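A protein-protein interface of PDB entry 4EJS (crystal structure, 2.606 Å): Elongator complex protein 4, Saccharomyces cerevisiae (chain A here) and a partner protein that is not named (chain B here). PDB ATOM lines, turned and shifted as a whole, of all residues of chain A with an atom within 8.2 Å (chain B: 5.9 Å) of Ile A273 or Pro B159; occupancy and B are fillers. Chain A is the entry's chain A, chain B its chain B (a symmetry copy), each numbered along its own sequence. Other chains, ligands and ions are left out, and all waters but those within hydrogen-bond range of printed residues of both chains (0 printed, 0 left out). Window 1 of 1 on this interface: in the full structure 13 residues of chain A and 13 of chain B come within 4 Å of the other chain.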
ATOM      1  N   GLU A  50     -10.539 -22.410   4.061  1.00  0.00           N
ATOM      2  CA  GLU A  50      -9.948 -22.126   2.762  1.00  0.00           C
ATOM      3  C   GLU A  50     -10.695 -21.026   2.014  1.00  0.00           C
ATOM      4  O   GLU A  50     -11.897 -20.848   2.203  1.00  0.00           O
ATOM      5  CB  GLU A  50      -9.883 -23.396   1.913  1.00  0.00           C
ATOM      6  CG  GLU A  50      -9.644 -23.116   0.433  1.00  0.00           C
ATOM      7  CD  GLU A  50      -8.801 -24.176  -0.239  1.00  0.00           C
ATOM      8  OE1 GLU A  50      -8.311 -25.070   0.485  1.00  0.00           O
ATOM      9  OE2 GLU A  50      -8.627 -24.114  -1.480  1.00  0.00           O
ATOM     10  N   GLN A  51      -9.975 -20.278   1.179  1.00  0.00           N
ATOM     11  CA  GLN A  51     -10.593 -19.296   0.294  1.00  0.00           C
ATOM     12  C   GLN A  51     -11.414 -20.017  -0.780  1.00  0.00           C
ATOM     13  O   GLN A  51     -11.397 -21.245  -0.865  1.00  0.00           O
ATOM     14  CB  GLN A  51      -9.532 -18.409  -0.341  1.00  0.00           C
ATOM     15  N   SER A  52     -12.129 -19.256  -1.600  1.00  0.00           N
ATOM     16  CA  SER A  52     -13.027 -19.845  -2.595  1.00  0.00           C
ATOM     17  C   SER A  52     -12.335 -20.806  -3.570  1.00  0.00           C
ATOM     18  O   SER A  52     -12.766 -21.953  -3.714  1.00  0.00           O
ATOM     19  CB  SER A  52     -13.776 -18.757  -3.353  1.00  0.00           C
ATOM     20  N   SER A 228     -17.137 -30.392   3.362  1.00  0.00           N
ATOM     21  CA  SER A 228     -17.231 -28.924   3.349  1.00  0.00           C
ATOM     22  C   SER A 228     -18.455 -28.381   4.075  1.00  0.00           C
ATOM     23  O   SER A 228     -19.523 -28.157   3.489  1.00  0.00           O
ATOM     24  CB  SER A 228     -17.045 -28.303   1.953  1.00  0.00           C
ATOM     25  OG  SER A 228     -18.118 -28.612   1.091  1.00  0.00           O
ATOM     26  N   LEU A 229     -18.264 -28.208   5.377  1.00  0.00           N
ATOM     27  CA  LEU A 229     -19.240 -27.592   6.236  1.00  0.00           C
ATOM     28  C   LEU A 229     -19.969 -26.451   5.528  1.00  0.00           C
ATOM     29  O   LEU A 229     -19.353 -25.505   5.026  1.00  0.00           O
ATOM     30  CB  LEU A 229     -18.550 -27.048   7.479  1.00  0.00           C
ATOM     31  CG  LEU A 229     -18.938 -27.687   8.802  1.00  0.00           C
ATOM     32  CD1 LEU A 229     -18.475 -26.765   9.906  1.00  0.00           C
ATOM     33  CD2 LEU A 229     -20.435 -27.922   8.885  1.00  0.00           C
ATOM     34  N   LEU A 230     -21.289 -26.564   5.494  1.00  0.00           N
ATOM     35  CA  LEU A 230     -22.170 -25.485   5.072  1.00  0.00           C
ATOM     36  C   LEU A 230     -22.096 -25.160   3.589  1.00  0.00           C
ATOM     37  O   LEU A 230     -22.503 -24.079   3.170  1.00  0.00           O
ATOM     38  CB  LEU A 230     -21.984 -24.236   5.946  1.00  0.00           C
ATOM     39  CG  LEU A 230     -22.623 -24.310   7.339  1.00  0.00           C
ATOM     40  CD1 LEU A 230     -22.214 -23.127   8.211  1.00  0.00           C
ATOM     41  CD2 LEU A 230     -24.146 -24.372   7.203  1.00  0.00           C
ATOM     42  N   HIS A 231     -21.593 -26.100   2.795  1.00  0.00           N
ATOM     43  CA  HIS A 231     -21.772 -25.985   1.364  1.00  0.00           C
ATOM     44  C   HIS A 231     -23.275 -25.839   1.094  1.00  0.00           C
ATOM     45  O   HIS A 231     -24.068 -26.710   1.466  1.00  0.00           O
ATOM     46  CB  HIS A 231     -21.228 -27.211   0.651  1.00  0.00           C
ATOM     47  CG  HIS A 231     -21.046 -27.004  -0.817  1.00  0.00           C
ATOM     48  ND1 HIS A 231     -22.093 -26.676  -1.655  1.00  0.00           N
ATOM     49  CD2 HIS A 231     -19.939 -27.049  -1.595  1.00  0.00           C
ATOM     50  CE1 HIS A 231     -21.638 -26.536  -2.888  1.00  0.00           C
ATOM     51  NE2 HIS A 231     -20.335 -26.754  -2.878  1.00  0.00           N
ATOM     52  N   PRO A 232     -23.675 -24.734   0.445  1.00  0.00           N
ATOM     53  CA  PRO A 232     -25.088 -24.387   0.245  1.00  0.00           C
ATOM     54  C   PRO A 232     -25.856 -25.400  -0.607  1.00  0.00           C
ATOM     55  O   PRO A 232     -27.088 -25.431  -0.549  1.00  0.00           O
ATOM     56  CB  PRO A 232     -25.017 -23.043  -0.489  1.00  0.00           C
ATOM     57  CG  PRO A 232     -23.630 -22.546  -0.287  1.00  0.00           C
ATOM     58  CD  PRO A 232     -22.776 -23.760  -0.190  1.00  0.00           C
ATOM     59  N   ALA A 233     -25.135 -26.189  -1.401  1.00  0.00           N
ATOM     60  CA  ALA A 233     -25.727 -27.249  -2.213  1.00  0.00           C
ATOM     61  C   ALA A 233     -26.016 -28.520  -1.407  1.00  0.00           C
ATOM     62  O   ALA A 233     -26.742 -29.393  -1.865  1.00  0.00           O
ATOM     63  CB  ALA A 233     -24.811 -27.590  -3.394  1.00  0.00           C
ATOM     64  N   TYR A 235     -26.295 -28.214   2.389  1.00  0.00           N
ATOM     65  CA  TYR A 235     -26.842 -27.819   3.677  1.00  0.00           C
ATOM     66  C   TYR A 235     -28.032 -26.905   3.442  1.00  0.00           C
ATOM     67  O   TYR A 235     -27.895 -25.841   2.846  1.00  0.00           O
ATOM     68  CB  TYR A 235     -25.761 -27.127   4.528  1.00  0.00           C
ATOM     69  CG  TYR A 235     -24.653 -28.060   5.012  1.00  0.00           C
ATOM     70  CD1 TYR A 235     -24.567 -28.443   6.348  1.00  0.00           C
ATOM     71  CD2 TYR A 235     -23.695 -28.561   4.129  1.00  0.00           C
ATOM     72  CE1 TYR A 235     -23.571 -29.310   6.789  1.00  0.00           C
ATOM     73  CE2 TYR A 235     -22.691 -29.421   4.564  1.00  0.00           C
ATOM     74  CZ  TYR A 235     -22.638 -29.794   5.891  1.00  0.00           C
ATOM     75  OH  TYR A 235     -21.638 -30.642   6.314  1.00  0.00           O
ATOM     76  N   PRO A 237     -31.054 -24.257   3.740  1.00  0.00           N
ATOM     77  CA  PRO A 237     -31.021 -22.894   4.290  1.00  0.00           C
ATOM     78  C   PRO A 237     -31.288 -22.853   5.794  1.00  0.00           C
ATOM     79  O   PRO A 237     -30.581 -22.151   6.530  1.00  0.00           O
ATOM     80  CB  PRO A 237     -32.148 -22.190   3.532  1.00  0.00           C
ATOM     81  CG  PRO A 237     -32.147 -22.894   2.185  1.00  0.00           C
ATOM     82  CD  PRO A 237     -31.802 -24.338   2.471  1.00  0.00           C
ATOM     83  N   PHE A 240     -28.660 -23.093   8.500  1.00  0.00           N
ATOM     84  CA  PHE A 240     -27.768 -21.961   8.701  1.00  0.00           C
ATOM     85  C   PHE A 240     -28.249 -21.128   9.878  1.00  0.00           C
ATOM     86  O   PHE A 240     -27.586 -20.182  10.287  1.00  0.00           O
ATOM     87  CB  PHE A 240     -27.698 -21.090   7.438  1.00  0.00           C
ATOM     88  CG  PHE A 240     -26.809 -21.640   6.357  1.00  0.00           C
ATOM     89  CD1 PHE A 240     -25.575 -21.054   6.090  1.00  0.00           C
ATOM     90  CD2 PHE A 240     -27.217 -22.718   5.585  1.00  0.00           C
ATOM     91  CE1 PHE A 240     -24.762 -21.541   5.076  1.00  0.00           C
ATOM     92  CE2 PHE A 240     -26.410 -23.215   4.564  1.00  0.00           C
ATOM     93  CZ  PHE A 240     -25.180 -22.633   4.313  1.00  0.00           C
ATOM     94  N   ILE A 269     -14.182 -25.837   5.446  1.00  0.00           N
ATOM     95  CA  ILE A 269     -15.223 -24.885   5.174  1.00  0.00           C
ATOM     96  C   ILE A 269     -14.654 -23.823   4.251  1.00  0.00           C
ATOM     97  O   ILE A 269     -13.476 -23.476   4.353  1.00  0.00           O
ATOM     98  CB  ILE A 269     -15.765 -24.285   6.495  1.00  0.00           C
ATOM     99  CG1 ILE A 269     -16.833 -23.230   6.217  1.00  0.00           C
ATOM    100  CG2 ILE A 269     -14.632 -23.726   7.345  1.00  0.00           C
ATOM    101  CD1 ILE A 269     -17.640 -22.887   7.430  1.00  0.00           C
ATOM    102  N   SER A 270     -15.479 -23.357   3.319  1.00  0.00           N
ATOM    103  CA  SER A 270     -15.130 -22.240   2.459  1.00  0.00           C
ATOM    104  C   SER A 270     -15.625 -20.944   3.091  1.00  0.00           C
ATOM    105  O   SER A 270     -16.830 -20.743   3.219  1.00  0.00           O
ATOM    106  CB  SER A 270     -15.780 -22.413   1.092  1.00  0.00           C
ATOM    107  OG  SER A 270     -15.121 -23.418   0.354  1.00  0.00           O
ATOM    108  N   ILE A 271     -14.689 -20.067   3.454  1.00  0.00           N
ATOM    109  CA  ILE A 271     -14.970 -18.833   4.189  1.00  0.00           C
ATOM    110  C   ILE A 271     -15.712 -17.738   3.402  1.00  0.00           C
ATOM    111  O   ILE A 271     -16.173 -16.747   3.977  1.00  0.00           O
ATOM    112  CB  ILE A 271     -13.661 -18.236   4.741  1.00  0.00           C
ATOM    113  CG1 ILE A 271     -12.935 -19.281   5.577  1.00  0.00           C
ATOM    114  CG2 ILE A 271     -13.937 -17.009   5.584  1.00  0.00           C
ATOM    115  CD1 ILE A 271     -13.860 -20.039   6.501  1.00  0.00           C
ATOM    116  N   ASP A 272     -15.829 -17.904   2.093  1.00  0.00           N
ATOM    117  CA  ASP A 272     -16.493 -16.886   1.279  1.00  0.00           C
ATOM    118  C   ASP A 272     -18.026 -16.921   1.392  1.00  0.00           C
ATOM    119  O   ASP A 272     -18.702 -15.920   1.146  1.00  0.00           O
ATOM    120  CB  ASP A 272     -16.001 -16.921  -0.184  1.00  0.00           C
ATOM    121  CG  ASP A 272     -15.848 -18.342  -0.735  1.00  0.00           C
ATOM    122  OD1 ASP A 272     -14.962 -19.091  -0.260  1.00  0.00           O
ATOM    123  OD2 ASP A 272     -16.599 -18.703  -1.667  1.00  0.00           O
ATOM    124  N   ILE A 273     -18.572 -18.064   1.798  1.00  0.00           N
ATOM    125  CA  ILE A 273     -20.010 -18.172   2.023  1.00  0.00           C
ATOM    126  C   ILE A 273     -20.429 -18.184   3.507  1.00  0.00           C
ATOM    127  O   ILE A 273     -21.590 -18.455   3.818  1.00  0.00           O
ATOM    128  CB  ILE A 273     -20.644 -19.370   1.243  1.00  0.00           C
ATOM    129  CG1 ILE A 273     -19.821 -20.651   1.401  1.00  0.00           C
ATOM    130  CG2 ILE A 273     -20.779 -19.036  -0.225  1.00  0.00           C
ATOM    131  CD1 ILE A 273     -20.305 -21.570   2.510  1.00  0.00           C
ATOM    132  N   ILE A 274     -19.498 -17.882   4.416  1.00  0.00           N
ATOM    133  CA  ILE A 274     -19.830 -17.762   5.846  1.00  0.00           C
ATOM    134  C   ILE A 274     -19.679 -16.326   6.357  1.00  0.00           C
ATOM    135  O   ILE A 274     -18.632 -15.701   6.190  1.00  0.00           O
ATOM    136  CB  ILE A 274     -18.961 -18.672   6.739  1.00  0.00           C
ATOM    137  CG1 ILE A 274     -18.501 -19.901   5.974  1.00  0.00           C
ATOM    138  CG2 ILE A 274     -19.740 -19.110   7.963  1.00  0.00           C
ATOM    139  CD1 ILE A 274     -19.604 -20.882   5.717  1.00  0.00           C
ATOM    140  N   THR A 275     -20.730 -15.800   6.974  1.00  0.00           N
ATOM    141  CA  THR A 275     -20.623 -14.515   7.648  1.00  0.00           C
ATOM    142  C   THR A 275     -19.660 -14.638   8.833  1.00  0.00           C
ATOM    143  O   THR A 275     -19.599 -15.677   9.483  1.00  0.00           O
ATOM    144  CB  THR A 275     -22.001 -13.997   8.143  1.00  0.00           C
ATOM    145  OG1 THR A 275     -22.748 -15.080   8.710  1.00  0.00           O
ATOM    146  CG2 THR A 275     -22.788 -13.396   7.006  1.00  0.00           C
ATOM    147  N   PRO A 276     -18.902 -13.573   9.115  1.00  0.00           N
ATOM    148  CA  PRO A 276     -17.921 -13.560  10.209  1.00  0.00           C
ATOM    149  C   PRO A 276     -18.483 -13.973  11.580  1.00  0.00           C
ATOM    150  O   PRO A 276     -17.813 -14.698  12.315  1.00  0.00           O
ATOM    151  CB  PRO A 276     -17.456 -12.104  10.229  1.00  0.00           C
ATOM    152  CG  PRO A 276     -17.616 -11.660   8.793  1.00  0.00           C
ATOM    153  CD  PRO A 276     -18.881 -12.321   8.334  1.00  0.00           C
ATOM    154  N   LEU A 278     -20.898 -16.094  12.263  1.00  0.00           N
ATOM    155  CA  LEU A 278     -21.068 -17.533  12.262  1.00  0.00           C
ATOM    156  C   LEU A 278     -19.700 -18.226  12.272  1.00  0.00           C
ATOM    157  O   LEU A 278     -19.487 -19.209  12.986  1.00  0.00           O
ATOM    158  CB  LEU A 278     -21.874 -17.953  11.045  1.00  0.00           C
ATOM    159  CG  LEU A 278     -22.282 -19.413  11.034  1.00  0.00           C
ATOM    160  CD1 LEU A 278     -23.043 -19.713  12.312  1.00  0.00           C
ATOM    161  CD2 LEU A 278     -23.119 -19.687   9.803  1.00  0.00           C
ATOM    162  N   LEU A 279     -18.763 -17.708  11.486  1.00  0.00           N
ATOM    163  CA  LEU A 279     -17.427 -18.270  11.476  1.00  0.00           C
ATOM    164  C   LEU A 279     -16.812 -18.249  12.879  1.00  0.00           C
ATOM    165  O   LEU A 279     -16.198 -19.236  13.303  1.00  0.00           O
ATOM    166  CB  LEU A 279     -16.557 -17.535  10.474  1.00  0.00           C
ATOM    167  CG  LEU A 279     -15.191 -18.170  10.274  1.00  0.00           C
ATOM    168  CD1 LEU A 279     -15.298 -19.678  10.025  1.00  0.00           C
ATOM    169  CD2 LEU A 279     -14.507 -17.475   9.134  1.00  0.00           C
ATOM    170  N   THR B 118     -34.110 -16.606  -2.329  1.00  0.00           N
ATOM    171  CA  THR B 118     -32.764 -17.032  -1.953  1.00  0.00           C
ATOM    172  C   THR B 118     -32.709 -18.489  -1.457  1.00  0.00           C
ATOM    173  O   THR B 118     -31.777 -19.228  -1.778  1.00  0.00           O
ATOM    174  CB  THR B 118     -32.175 -16.060  -0.907  1.00  0.00           C
ATOM    175  OG1 THR B 118     -32.186 -14.740  -1.460  1.00  0.00           O
ATOM    176  CG2 THR B 118     -30.738 -16.437  -0.543  1.00  0.00           C
ATOM    177  N   ASP B 145     -31.996  -7.764  -1.903  1.00  0.00           N
ATOM    178  CA  ASP B 145     -32.892  -8.888  -1.565  1.00  0.00           C
ATOM    179  C   ASP B 145     -34.106  -8.463  -0.717  1.00  0.00           C
ATOM    180  O   ASP B 145     -35.248  -8.872  -0.981  1.00  0.00           O
ATOM    181  CB  ASP B 145     -32.128 -10.043  -0.891  1.00  0.00           C
ATOM    182  CG  ASP B 145     -30.952 -10.549  -1.732  1.00  0.00           C
ATOM    183  OD1 ASP B 145     -30.989 -10.393  -2.978  1.00  0.00           O
ATOM    184  OD2 ASP B 145     -29.988 -11.106  -1.143  1.00  0.00           O
ATOM    185  N   ASN B 155     -32.006 -16.392   7.573  1.00  0.00           N
ATOM    186  CA  ASN B 155     -31.661 -15.485   6.481  1.00  0.00           C
ATOM    187  C   ASN B 155     -30.449 -14.688   6.895  1.00  0.00           C
ATOM    188  O   ASN B 155     -29.560 -14.381   6.087  1.00  0.00           O
ATOM    189  CB  ASN B 155     -32.832 -14.556   6.154  1.00  0.00           C
ATOM    190  N   ASN B 157     -27.823 -15.590   8.664  1.00  0.00           N
ATOM    191  CA  ASN B 157     -26.561 -16.309   8.433  1.00  0.00           C
ATOM    192  C   ASN B 157     -26.383 -16.890   7.045  1.00  0.00           C
ATOM    193  O   ASN B 157     -25.260 -17.206   6.628  1.00  0.00           O
ATOM    194  CB  ASN B 157     -26.426 -17.458   9.407  1.00  0.00           C
ATOM    195  CG  ASN B 157     -26.357 -17.003  10.817  1.00  0.00           C
ATOM    196  OD1 ASN B 157     -26.068 -15.829  11.092  1.00  0.00           O
ATOM    197  ND2 ASN B 157     -26.613 -17.928  11.743  1.00  0.00           N
ATOM    198  N   TYR B 158     -27.501 -17.069   6.353  1.00  0.00           N
ATOM    199  CA  TYR B 158     -27.475 -17.625   5.024  1.00  0.00           C
ATOM    200  C   TYR B 158     -26.837 -16.600   4.083  1.00  0.00           C
ATOM    201  O   TYR B 158     -27.091 -15.397   4.206  1.00  0.00           O
ATOM    202  CB  TYR B 158     -28.897 -18.023   4.579  1.00  0.00           C
ATOM    203  CG  TYR B 158     -28.879 -18.991   3.417  1.00  0.00           C
ATOM    204  CD1 TYR B 158     -28.397 -20.293   3.582  1.00  0.00           C
ATOM    205  CD2 TYR B 158     -29.307 -18.601   2.148  1.00  0.00           C
ATOM    206  CE1 TYR B 158     -28.347 -21.173   2.523  1.00  0.00           C
ATOM    207  CE2 TYR B 158     -29.271 -19.488   1.087  1.00  0.00           C
ATOM    208  CZ  TYR B 158     -28.783 -20.770   1.277  1.00  0.00           C
ATOM    209  OH  TYR B 158     -28.738 -21.653   0.229  1.00  0.00           O
ATOM    210  N   PRO B 159     -25.995 -17.067   3.153  1.00  0.00           N
ATOM    211  CA  PRO B 159     -25.341 -16.099   2.252  1.00  0.00           C
ATOM    212  C   PRO B 159     -26.345 -15.303   1.407  1.00  0.00           C
ATOM    213  O   PRO B 159     -27.404 -15.819   1.054  1.00  0.00           O
ATOM    214  CB  PRO B 159     -24.406 -16.967   1.378  1.00  0.00           C
ATOM    215  CG  PRO B 159     -24.772 -18.403   1.674  1.00  0.00           C
ATOM    216  CD  PRO B 159     -25.483 -18.444   2.997  1.00  0.00           C
ATOM    217  N   ASP B 160     -26.031 -14.041   1.121  1.00  0.00           N
ATOM    218  CA  ASP B 160     -26.900 -13.211   0.280  1.00  0.00           C
ATOM    219  C   ASP B 160     -26.901 -13.729  -1.165  1.00  0.00           C
ATOM    220  O   ASP B 160     -25.991 -14.462  -1.585  1.00  0.00           O
ATOM    221  CB  ASP B 160     -26.431 -11.762   0.311  1.00  0.00           C
ATOM    222  CG  ASP B 160     -24.940 -11.649   0.115  1.00  0.00           C
ATOM    223  OD1 ASP B 160     -24.510 -11.564  -1.052  1.00  0.00           O
ATOM    224  OD2 ASP B 160     -24.197 -11.689   1.126  1.00  0.00           O
ATOM    225  N   LYS B 161     -27.917 -13.354  -1.933  1.00  0.00           N
ATOM    226  CA  LYS B 161     -28.081 -13.958  -3.251  1.00  0.00           C
ATOM    227  C   LYS B 161     -26.804 -13.877  -4.103  1.00  0.00           C
ATOM    228  O   LYS B 161     -26.404 -14.857  -4.717  1.00  0.00           O
ATOM    229  CB  LYS B 161     -29.311 -13.399  -3.982  1.00  0.00           C
ATOM    230  CG  LYS B 161     -29.906 -14.379  -4.973  1.00  0.00           C
ATOM    231  CD  LYS B 161     -31.223 -13.866  -5.517  1.00  0.00           C
ATOM    232  CE  LYS B 161     -32.233 -13.736  -4.414  1.00  0.00           C
ATOM    233  NZ  LYS B 161     -33.483 -13.182  -4.945  1.00  0.00           N
ATOM    234  N   THR B 163     -23.452 -13.434  -3.289  1.00  0.00           N
ATOM    235  CA  THR B 163     -22.366 -14.283  -2.778  1.00  0.00           C
ATOM    236  C   THR B 163     -22.614 -15.743  -3.117  1.00  0.00           C
ATOM    237  O   THR B 163     -21.709 -16.472  -3.528  1.00  0.00           O
ATOM    238  CB  THR B 163     -22.260 -14.185  -1.251  1.00  0.00           C
ATOM    239  OG1 THR B 163     -21.939 -12.843  -0.893  1.00  0.00           O
ATOM    240  CG2 THR B 163     -21.180 -15.146  -0.696  1.00  0.00           C
ATOM    241  N   LEU B 164     -23.863 -16.146  -2.927  1.00  0.00           N
ATOM    242  CA  LEU B 164     -24.332 -17.480  -3.245  1.00  0.00           C
ATOM    243  C   LEU B 164     -24.151 -17.797  -4.725  1.00  0.00           C
ATOM    244  O   LEU B 164     -23.561 -18.812  -5.087  1.00  0.00           O
ATOM    245  CB  LEU B 164     -25.811 -17.592  -2.862  1.00  0.00           C
ATOM    246  CG  LEU B 164     -26.446 -18.963  -3.054  1.00  0.00           C
ATOM    247  CD1 LEU B 164     -25.612 -19.978  -2.321  1.00  0.00           C
ATOM    248  CD2 LEU B 164     -27.881 -18.962  -2.568  1.00  0.00           C
ATOM    249  N   PHE B 167     -20.644 -18.200  -5.964  1.00  0.00           N
ATOM    250  CA  PHE B 167     -20.126 -19.463  -5.452  1.00  0.00           C
ATOM    251  C   PHE B 167     -20.586 -20.673  -6.282  1.00  0.00           C
ATOM    252  O   PHE B 167     -19.802 -21.586  -6.543  1.00  0.00           O
ATOM    253  CB  PHE B 167     -20.538 -19.629  -3.979  1.00  0.00           C
ATOM    254  CG  PHE B 167     -20.069 -20.912  -3.358  1.00  0.00           C
ATOM    255  CD1 PHE B 167     -18.782 -21.026  -2.850  1.00  0.00           C
ATOM    256  CD2 PHE B 167     -20.911 -22.009  -3.281  1.00  0.00           C
ATOM    257  CE1 PHE B 167     -18.345 -22.213  -2.281  1.00  0.00           C
ATOM    258  CE2 PHE B 167     -20.476 -23.203  -2.712  1.00  0.00           C
ATOM    259  CZ  PHE B 167     -19.196 -23.306  -2.216  1.00  0.00           C
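His A231 touches Phe B167. Pro A232 touches Leu B164 (CB to CD1, 3.6 Å). CA of Pro A237 touches CE1 of Tyr B158, at 3.6 Å. CE1 of Phe A240 touches CD of Pro B159, 3.8 Å away. Thr B163 touches Asp A272. OD2 of Asp A272 touches CD1 of Phe B167, at 3.4 Å. CG of Pro B159 touches O of Ile A273 (3.8 Å). Ile A273 touches Thr B163 (CG2 to CG2, 3.9 Å). Ile A273 touches Phe B167. O of Asn B157 touches OG1 of Thr A275 (3.9 Å).
The backbone carbonyl oxygen (O) of Phe A240 sits at hydrogen-bond distance from the side-chain amide nitrogen (ND2) of Asn B157, 2.9 Å away.
The backbone NH (N) of Ser A52 sits close to the side-chain carboxylate (OD1) of Asp A272, 3.1 Å away. ND1 of His A231 is in hydrogen-bond range of N of Ala A233, at 3.1 Å. OG1 of Thr B163 sits at hydrogen-bond distance from OD1 of Asp B160 (2.9 Å).
Printed residues of chain B within 4 Å of His A231: Phe B167 (3.5 Å). Of the printed residues of chain B, Pro A232 touches Leu B164 (3.6 Å) and Phe B167 (3.5 Å). Of chain B, only Pro B159 (3.8 Å), Thr B163 (3.9 Å) and Phe B167 (3.7 Å) come within 4 Å of Ile A273. The nearest residue of chain B that does not touch Ile A273 is Asn B157 (4.8 Å).
Of the 11 printed residues of chain B, 6 touch a printed residue of chain A.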
